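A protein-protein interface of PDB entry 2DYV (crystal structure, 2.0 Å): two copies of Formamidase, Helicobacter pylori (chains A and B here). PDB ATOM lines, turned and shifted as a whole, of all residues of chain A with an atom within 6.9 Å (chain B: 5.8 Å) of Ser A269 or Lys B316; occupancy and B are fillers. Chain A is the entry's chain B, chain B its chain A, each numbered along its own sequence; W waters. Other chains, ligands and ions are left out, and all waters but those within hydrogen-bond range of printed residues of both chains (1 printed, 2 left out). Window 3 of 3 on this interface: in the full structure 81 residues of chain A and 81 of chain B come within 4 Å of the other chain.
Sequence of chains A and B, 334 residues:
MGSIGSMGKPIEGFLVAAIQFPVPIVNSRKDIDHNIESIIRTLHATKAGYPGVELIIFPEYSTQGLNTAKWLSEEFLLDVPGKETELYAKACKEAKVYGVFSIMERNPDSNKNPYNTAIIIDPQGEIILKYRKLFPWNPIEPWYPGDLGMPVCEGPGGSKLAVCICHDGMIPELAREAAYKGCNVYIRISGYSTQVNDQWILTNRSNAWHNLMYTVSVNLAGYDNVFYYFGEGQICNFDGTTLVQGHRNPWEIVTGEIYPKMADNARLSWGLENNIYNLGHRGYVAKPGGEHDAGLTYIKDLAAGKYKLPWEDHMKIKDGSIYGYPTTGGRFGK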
ATOM      1  N   ASP A 264       6.508 -26.552 -28.976  1.00  0.00           N
ATOM      2  CA  ASP A 264       5.550 -25.536 -28.518  1.00  0.00           C
ATOM      3  C   ASP A 264       4.279 -26.175 -27.964  1.00  0.00           C
ATOM      4  O   ASP A 264       3.778 -25.732 -26.931  1.00  0.00           O
ATOM      5  CB  ASP A 264       5.153 -24.582 -29.643  1.00  0.00           C
ATOM      6  CG  ASP A 264       6.294 -23.695 -30.104  1.00  0.00           C
ATOM      7  OD1 ASP A 264       7.379 -23.719 -29.488  1.00  0.00           O
ATOM      8  OD2 ASP A 264       6.089 -22.957 -31.102  1.00  0.00           O
ATOM      9  N   ASN A 265       3.771 -27.202 -28.657  1.00  0.00           N
ATOM     10  CA  ASN A 265       2.524 -27.879 -28.276  1.00  0.00           C
ATOM     11  C   ASN A 265       2.653 -28.688 -27.006  1.00  0.00           C
ATOM     12  O   ASN A 265       1.705 -28.776 -26.236  1.00  0.00           O
ATOM     13  CB  ASN A 265       1.995 -28.761 -29.422  1.00  0.00           C
ATOM     14  CG  ASN A 265       1.486 -27.939 -30.594  1.00  0.00           C
ATOM     15  OD1 ASN A 265       1.351 -26.718 -30.490  1.00  0.00           O
ATOM     16  ND2 ASN A 265       1.209 -28.600 -31.714  1.00  0.00           N
ATOM     17  N   ALA A 266       3.826 -29.280 -26.801  1.00  0.00           N
ATOM     18  CA  ALA A 266       4.165 -29.941 -25.545  1.00  0.00           C
ATOM     19  C   ALA A 266       4.113 -28.917 -24.410  1.00  0.00           C
ATOM     20  O   ALA A 266       3.497 -29.162 -23.385  1.00  0.00           O
ATOM     21  CB  ALA A 266       5.563 -30.593 -25.633  1.00  0.00           C
ATOM     22  N   ARG A 267       4.743 -27.761 -24.610  1.00  0.00           N
ATOM     23  CA  ARG A 267       4.705 -26.686 -23.615  1.00  0.00           C
ATOM     24  C   ARG A 267       3.276 -26.201 -23.351  1.00  0.00           C
ATOM     25  O   ARG A 267       2.917 -25.888 -22.212  1.00  0.00           O
ATOM     26  CB  ARG A 267       5.567 -25.516 -24.071  1.00  0.00           C
ATOM     27  CG  ARG A 267       7.056 -25.796 -23.970  1.00  0.00           C
ATOM     28  CD  ARG A 267       7.835 -24.779 -24.770  1.00  0.00           C
ATOM     29  NE  ARG A 267       9.265 -24.893 -24.482  1.00  0.00           N
ATOM     30  CZ  ARG A 267      10.192 -24.061 -24.941  1.00  0.00           C
ATOM     31  NH1 ARG A 267       9.844 -23.033 -25.714  1.00  0.00           N
ATOM     32  NH2 ARG A 267      11.472 -24.256 -24.617  1.00  0.00           N
ATOM     33  N   LEU A 268       2.464 -26.154 -24.404  1.00  0.00           N
ATOM     34  CA  LEU A 268       1.064 -25.730 -24.253  1.00  0.00           C
ATOM     35  C   LEU A 268       0.169 -26.759 -23.594  1.00  0.00           C
ATOM     36  O   LEU A 268      -0.715 -26.403 -22.825  1.00  0.00           O
ATOM     37  CB  LEU A 268       0.465 -25.306 -25.601  1.00  0.00           C
ATOM     38  CG  LEU A 268       1.019 -24.005 -26.206  1.00  0.00           C
ATOM     39  CD1 LEU A 268       0.395 -23.703 -27.580  1.00  0.00           C
ATOM     40  CD2 LEU A 268       0.833 -22.837 -25.258  1.00  0.00           C
ATOM     41  N   SER A 269       0.413 -28.033 -23.884  1.00  0.00           N
ATOM     42  CA  SER A 269      -0.563 -29.089 -23.606  1.00  0.00           C
ATOM     43  C   SER A 269      -0.237 -29.967 -22.409  1.00  0.00           C
ATOM     44  O   SER A 269      -1.142 -30.496 -21.770  1.00  0.00           O
ATOM     45  CB  SER A 269      -0.733 -29.984 -24.832  1.00  0.00           C
ATOM     46  OG  SER A 269      -1.266 -29.235 -25.901  1.00  0.00           O
ATOM     47  N   TRP A 270       1.047 -30.130 -22.111  1.00  0.00           N
ATOM     48  CA  TRP A 270       1.441 -31.111 -21.106  1.00  0.00           C
ATOM     49  C   TRP A 270       1.195 -30.652 -19.677  1.00  0.00           C
ATOM     50  O   TRP A 270       1.189 -29.455 -19.392  1.00  0.00           O
ATOM     51  CB  TRP A 270       2.895 -31.571 -21.316  1.00  0.00           C
ATOM     52  CG  TRP A 270       3.060 -32.462 -22.537  1.00  0.00           C
ATOM     53  CD1 TRP A 270       2.061 -32.939 -23.345  1.00  0.00           C
ATOM     54  CD2 TRP A 270       4.281 -33.008 -23.051  1.00  0.00           C
ATOM     55  NE1 TRP A 270       2.587 -33.729 -24.339  1.00  0.00           N
ATOM     56  CE2 TRP A 270       3.948 -33.787 -24.186  1.00  0.00           C
ATOM     57  CE3 TRP A 270       5.627 -32.906 -22.674  1.00  0.00           C
ATOM     58  CZ2 TRP A 270       4.918 -34.471 -24.949  1.00  0.00           C
ATOM     59  CZ3 TRP A 270       6.597 -33.580 -23.434  1.00  0.00           C
ATOM     60  CH2 TRP A 270       6.230 -34.358 -24.554  1.00  0.00           C
ATOM     61  N   GLY A 271       0.968 -31.623 -18.793  1.00  0.00           N
ATOM     62  CA  GLY A 271       0.818 -31.361 -17.360  1.00  0.00           C
ATOM     63  C   GLY A 271       1.987 -31.920 -16.567  1.00  0.00           C
ATOM     64  O   GLY A 271       2.851 -31.164 -16.086  1.00  0.00           O
ATOM     65  N   LEU A 272       2.037 -33.247 -16.460  1.00  0.00           N
ATOM     66  CA  LEU A 272       3.027 -33.914 -15.620  1.00  0.00           C
ATOM     67  C   LEU A 272       4.470 -33.592 -16.020  1.00  0.00           C
ATOM     68  O   LEU A 272       5.354 -33.469 -15.164  1.00  0.00           O
ATOM     69  CB  LEU A 272       2.779 -35.434 -15.598  1.00  0.00           C
ATOM     70  CG  LEU A 272       1.410 -35.884 -15.065  1.00  0.00           C
ATOM     71  CD1 LEU A 272       1.267 -37.406 -15.187  1.00  0.00           C
ATOM     72  CD2 LEU A 272       1.167 -35.447 -13.640  1.00  0.00           C
ATOM     73  N   GLU A 273       4.688 -33.431 -17.318  1.00  0.00           N
ATOM     74  CA  GLU A 273       6.013 -33.162 -17.874  1.00  0.00           C
ATOM     75  C   GLU A 273       6.401 -31.674 -17.917  1.00  0.00           C
ATOM     76  O   GLU A 273       7.486 -31.317 -18.414  1.00  0.00           O
ATOM     77  CB  GLU A 273       6.081 -33.730 -19.301  1.00  0.00           C
ATOM     78  CG  GLU A 273       5.734 -35.218 -19.422  1.00  0.00           C
ATOM     79  CD  GLU A 273       4.227 -35.495 -19.591  1.00  0.00           C
ATOM     80  OE1 GLU A 273       3.378 -34.580 -19.411  1.00  0.00           O
ATOM     81  OE2 GLU A 273       3.901 -36.655 -19.917  1.00  0.00           O
ATOM     82  N   ASN A 274       5.523 -30.797 -17.436  1.00  0.00           N
ATOM     83  CA  ASN A 274       5.723 -29.379 -17.718  1.00  0.00           C
ATOM     84  C   ASN A 274       6.558 -28.667 -16.654  1.00  0.00           C
ATOM     85  O   ASN A 274       6.096 -27.724 -16.008  1.00  0.00           O
ATOM     86  CB  ASN A 274       4.392 -28.668 -17.975  1.00  0.00           C
ATOM     87  CG  ASN A 274       4.522 -27.542 -18.973  1.00  0.00           C
ATOM     88  OD1 ASN A 274       5.480 -26.771 -18.937  1.00  0.00           O
ATOM     89  ND2 ASN A 274       3.561 -27.451 -19.887  1.00  0.00           N
ATOM     90  N   HIS B 314      -1.908 -19.498 -23.394  1.00  0.00           N
ATOM     91  CA  HIS B 314      -2.569 -20.540 -24.169  1.00  0.00           C
ATOM     92  C   HIS B 314      -2.379 -21.952 -23.593  1.00  0.00           C
ATOM     93  O   HIS B 314      -2.641 -22.938 -24.286  1.00  0.00           O
ATOM     94  CB  HIS B 314      -2.105 -20.490 -25.634  1.00  0.00           C
ATOM     95  CG  HIS B 314      -2.375 -19.179 -26.315  1.00  0.00           C
ATOM     96  ND1 HIS B 314      -3.496 -18.957 -27.089  1.00  0.00           N
ATOM     97  CD2 HIS B 314      -1.674 -18.021 -26.330  1.00  0.00           C
ATOM     98  CE1 HIS B 314      -3.470 -17.720 -27.556  1.00  0.00           C
ATOM     99  NE2 HIS B 314      -2.374 -17.132 -27.110  1.00  0.00           N
ATOM    100  N   MET B 315      -1.947 -22.055 -22.337  1.00  0.00           N
ATOM    101  CA  MET B 315      -1.700 -23.372 -21.726  1.00  0.00           C
ATOM    102  C   MET B 315      -2.985 -24.066 -21.310  1.00  0.00           C
ATOM    103  O   MET B 315      -3.920 -23.416 -20.837  1.00  0.00           O
ATOM    104  CB  MET B 315      -0.757 -23.266 -20.528  1.00  0.00           C
ATOM    105  CG  MET B 315       0.721 -23.194 -20.918  1.00  0.00           C
ATOM    106  SD  MET B 315       1.784 -23.087 -19.471  1.00  0.00           S
ATOM    107  CE  MET B 315       1.419 -24.662 -18.686  1.00  0.00           C
ATOM    108  N   LYS B 316      -3.006 -25.390 -21.458  1.00  0.00           N
ATOM    109  CA  LYS B 316      -4.216 -26.177 -21.220  1.00  0.00           C
ATOM    110  C   LYS B 316      -4.365 -26.632 -19.780  1.00  0.00           C
ATOM    111  O   LYS B 316      -5.483 -26.790 -19.296  1.00  0.00           O
ATOM    112  CB  LYS B 316      -4.255 -27.418 -22.133  1.00  0.00           C
ATOM    113  CG  LYS B 316      -4.435 -27.118 -23.616  1.00  0.00           C
ATOM    114  CD  LYS B 316      -4.485 -28.419 -24.400  1.00  0.00           C
ATOM    115  CE  LYS B 316      -4.547 -28.193 -25.903  1.00  0.00           C
ATOM    116  NZ  LYS B 316      -4.296 -29.516 -26.584  1.00  0.00           N
ATOM    117  N   ILE B 317      -3.246 -26.881 -19.106  1.00  0.00           N
ATOM    118  CA  ILE B 317      -3.288 -27.445 -17.750  1.00  0.00           C
ATOM    119  C   ILE B 317      -2.618 -26.526 -16.718  1.00  0.00           C
ATOM    120  O   ILE B 317      -1.383 -26.451 -16.618  1.00  0.00           O
ATOM    121  CB  ILE B 317      -2.710 -28.881 -17.697  1.00  0.00           C
ATOM    122  CG1 ILE B 317      -3.460 -29.787 -18.688  1.00  0.00           C
ATOM    123  CG2 ILE B 317      -2.805 -29.431 -16.258  1.00  0.00           C
ATOM    124  CD1 ILE B 317      -2.913 -31.200 -18.818  1.00  0.00           C
ATOM    125  N   LYS B 318      -3.452 -25.814 -15.968  1.00  0.00           N
ATOM    126  CA  LYS B 318      -2.969 -24.852 -14.993  1.00  0.00           C
ATOM    127  C   LYS B 318      -3.681 -25.019 -13.656  1.00  0.00           C
ATOM    128  O   LYS B 318      -3.515 -24.207 -12.744  1.00  0.00           O
ATOM    129  CB  LYS B 318      -3.125 -23.424 -15.530  1.00  0.00           C
ATOM    130  CG  LYS B 318      -2.253 -23.129 -16.762  1.00  0.00           C
ATOM    131  CD  LYS B 318      -2.184 -21.631 -17.074  1.00  0.00           C
ATOM    132  CE  LYS B 318      -3.432 -21.141 -17.779  1.00  0.00           C
ATOM    133  NZ  LYS B 318      -3.269 -19.717 -18.218  1.00  0.00           N
HETATM  134  O   HOH W   1      -0.573 -27.321 -20.181  1.00  0.00           O
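Of chain A, only Leu A268 and Ser A269 come within 4 Å of Lys B316. Printed residues of chain A within 4 Å of Met B315: Arg A267, Leu A268 and Asn A274. Printed residues of chain A within 4 Å of His B314: Leu A268. Lys B318 touches none of the printed residues of chain A. Glu A273 touches none of the printed residues of chain B.
No position is printed for both chains.
O of Leu A268 sits at hydrogen-bond distance from N of Lys B316. The side-chain hydroxyl (OG) of Ser A269 lies within hydrogen-bond range of the side-chain amino group (NZ) of Lys B316, 3.1 Å away.
Among the printed residues, pairs that only touch across the chains: Leu A268 with Met B315 (3.4 Å), Ser A269 with Ile B317 (3.5 Å), Leu A268 with His B314 (3.6 Å), Arg A267 with Met B315 (3.7 Å), Asn A274 with Met B315 (3.7 Å) and Gly A271 with Ile B317 (3.9 Å).
The side-chain amide nitrogen (ND2) of Asn A274 lies within hydrogen-bond range of the backbone carbonyl oxygen (O) of Arg A267, at 2.9 Å. The backbone carbonyl oxygen (O) of Trp A270 is in hydrogen-bond range of the side-chain amide nitrogen (ND2) of Asn A274 (3.1 Å). OG of Ser A269 is in hydrogen-bond range of O of Asn A265, 3.0 Å away.
Water W1 lies within hydrogen-bond range of the backbone carbonyl oxygen of Leu A268 (2.8 Å), the backbone carbonyl oxygen of Trp A270 (2.9 Å), the backbone NH of Ile B317 (2.9 Å) and the backbone NH of Lys B316 (3.4 Å).
Of the 5 printed residues of chain B, 4 touch a printed residue of chain A. Of the 11 printed residues of chain A, 5 touch a printed residue of chain B. Printed residues of chain A that touch a printed residue of chain B: Arg A267, Leu A268, Ser A269, Gly A271 and Asn A274. Hydrophobic or aromatic side chains of chain A within 4 Å of the printed part of chain B: Leu A268. Among the printed residues, no Asp or Glu carboxylate lies within 4 Å of a Lys or Arg side-chain nitrogen of the other chain.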
